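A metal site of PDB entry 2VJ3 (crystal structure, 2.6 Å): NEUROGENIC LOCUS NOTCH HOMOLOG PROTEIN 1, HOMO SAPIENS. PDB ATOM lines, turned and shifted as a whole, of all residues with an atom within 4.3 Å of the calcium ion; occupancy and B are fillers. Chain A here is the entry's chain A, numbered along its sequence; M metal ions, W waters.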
ATOM      1  N   ASN A  82      13.516 -16.436  22.617  1.00  0.00           N
ATOM      2  CA  ASN A  82      12.234 -16.004  22.096  1.00  0.00           C
ATOM      3  C   ASN A  82      12.500 -14.876  21.102  1.00  0.00           C
ATOM      4  O   ASN A  82      12.738 -13.740  21.489  1.00  0.00           O
ATOM      5  CB  ASN A  82      11.323 -15.530  23.230  1.00  0.00           C
ATOM      6  CG  ASN A  82       9.859 -15.406  22.817  1.00  0.00           C
ATOM      7  OD1 ASN A  82       9.542 -15.033  21.685  1.00  0.00           O
ATOM      8  ND2 ASN A  82       8.964 -15.694  23.750  1.00  0.00           N
ATOM      9  N   THR A  83      12.460 -15.230  19.811  1.00  0.00           N
ATOM     10  CA  THR A  83      12.785 -14.306  18.720  1.00  0.00           C
ATOM     11  C   THR A  83      12.112 -12.945  18.890  1.00  0.00           C
ATOM     12  O   THR A  83      10.894 -12.864  19.078  1.00  0.00           O
ATOM     13  CB  THR A  83      12.378 -14.914  17.345  1.00  0.00           C
ATOM     14  OG1 THR A  83      13.013 -16.189  17.182  1.00  0.00           O
ATOM     15  CG2 THR A  83      12.799 -14.005  16.202  1.00  0.00           C
ATOM     16  N   GLU A  85      10.713 -10.102  17.280  1.00  0.00           N
ATOM     17  CA  GLU A  85      10.173  -9.677  15.987  1.00  0.00           C
ATOM     18  C   GLU A  85      10.258  -8.164  15.776  1.00  0.00           C
ATOM     19  O   GLU A  85      10.056  -7.670  14.657  1.00  0.00           O
ATOM     20  CB  GLU A  85       8.725 -10.155  15.820  1.00  0.00           C
ATOM     21  CG  GLU A  85       8.579 -11.564  15.261  1.00  0.00           C
ATOM     22  CD  GLU A  85       8.838 -12.649  16.292  1.00  0.00           C
ATOM     23  OE1 GLU A  85       8.489 -12.464  17.481  1.00  0.00           O
ATOM     24  OE2 GLU A  85       9.395 -13.707  15.919  1.00  0.00           O
ATOM     25  N   ASP A  99       6.407  -7.398  21.334  1.00  0.00           N
ATOM     26  CA  ASP A  99       6.851  -8.728  20.957  1.00  0.00           C
ATOM     27  C   ASP A  99       5.878  -9.822  21.415  1.00  0.00           C
ATOM     28  O   ASP A  99       5.400  -9.796  22.552  1.00  0.00           O
ATOM     29  CB  ASP A  99       8.250  -8.997  21.511  1.00  0.00           C
ATOM     30  CG  ASP A  99       8.824 -10.330  21.059  1.00  0.00           C
ATOM     31  OD1 ASP A  99       8.889 -10.569  19.839  1.00  0.00           O
ATOM     32  OD2 ASP A  99       9.220 -11.135  21.927  1.00  0.00           O
ATOM     33  N   LYS A 100       5.596 -10.759  20.515  1.00  0.00           N
ATOM     34  CA  LYS A 100       4.767 -11.928  20.808  1.00  0.00           C
ATOM     35  C   LYS A 100       5.513 -13.195  20.402  1.00  0.00           C
ATOM     36  O   LYS A 100       6.742 -13.184  20.304  1.00  0.00           O
ATOM     37  CB  LYS A 100       3.405 -11.833  20.100  1.00  0.00           C
ATOM     38  CG  LYS A 100       2.552 -10.615  20.483  1.00  0.00           C
ATOM     39  CD  LYS A 100       2.021 -10.727  21.916  1.00  0.00           C
ATOM     40  CE  LYS A 100       1.232  -9.483  22.308  1.00  0.00           C
ATOM     41  NZ  LYS A 100       0.787  -9.540  23.726  1.00  0.00           N
ATOM     42  N   ILE A 101       4.793 -14.288  20.157  1.00  0.00           N
ATOM     43  CA  ILE A 101       5.418 -15.529  19.678  1.00  0.00           C
ATOM     44  C   ILE A 101       5.200 -15.694  18.177  1.00  0.00           C
ATOM     45  O   ILE A 101       4.063 -15.824  17.720  1.00  0.00           O
ATOM     46  CB  ILE A 101       4.939 -16.780  20.471  1.00  0.00           C
ATOM     47  CG1 ILE A 101       5.355 -16.662  21.944  1.00  0.00           C
ATOM     48  CG2 ILE A 101       5.490 -18.054  19.838  1.00  0.00           C
ATOM     49  CD1 ILE A 101       4.952 -17.833  22.803  1.00  0.00           C
ATOM     50  N   ASN A 102       6.306 -15.687  17.428  1.00  0.00           N
ATOM     51  CA  ASN A 102       6.294 -15.682  15.958  1.00  0.00           C
ATOM     52  C   ASN A 102       5.377 -14.595  15.401  1.00  0.00           C
ATOM     53  O   ASN A 102       4.758 -14.746  14.338  1.00  0.00           O
ATOM     54  CB  ASN A 102       5.907 -17.054  15.406  1.00  0.00           C
ATOM     55  CG  ASN A 102       6.419 -17.291  13.988  1.00  0.00           C
ATOM     56  OD1 ASN A 102       7.352 -16.630  13.530  1.00  0.00           O
ATOM     57  ND2 ASN A 102       5.806 -18.251  13.295  1.00  0.00           N
HETATM   58 CA    CA M   1       8.875 -13.364  19.881  1.00  0.00          CA
HETATM   59  O   HOH W   1       9.225 -15.561  18.719  1.00  0.00           O
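Five residues have an atom within 4 Å of the calcium ion: Asn 82, Thr 83, Glu 85, Asp 99 and Lys 100. The nearest printed residue that does not touch the calcium ion is Ile 101 (4.1 Å).
The calcium ion is bound by O of Lys 100 (2.2 Å), O of Thr 83 (2.2 Å), water W1 (2.5 Å), OD1 of Asn 82 (2.5 Å), OE1 of Glu 85 (2.6 Å) and OD1 of Asp 99 (2.8 Å). The calcium ion has six donor atoms within binding distance. Slightly farther from the calcium ion lies OD2 of Asp 99 (3.0 Å).
Water W1 lies within hydrogen-bond range of N of Asn 102, OE2 of Glu 85 and N of Thr 83.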
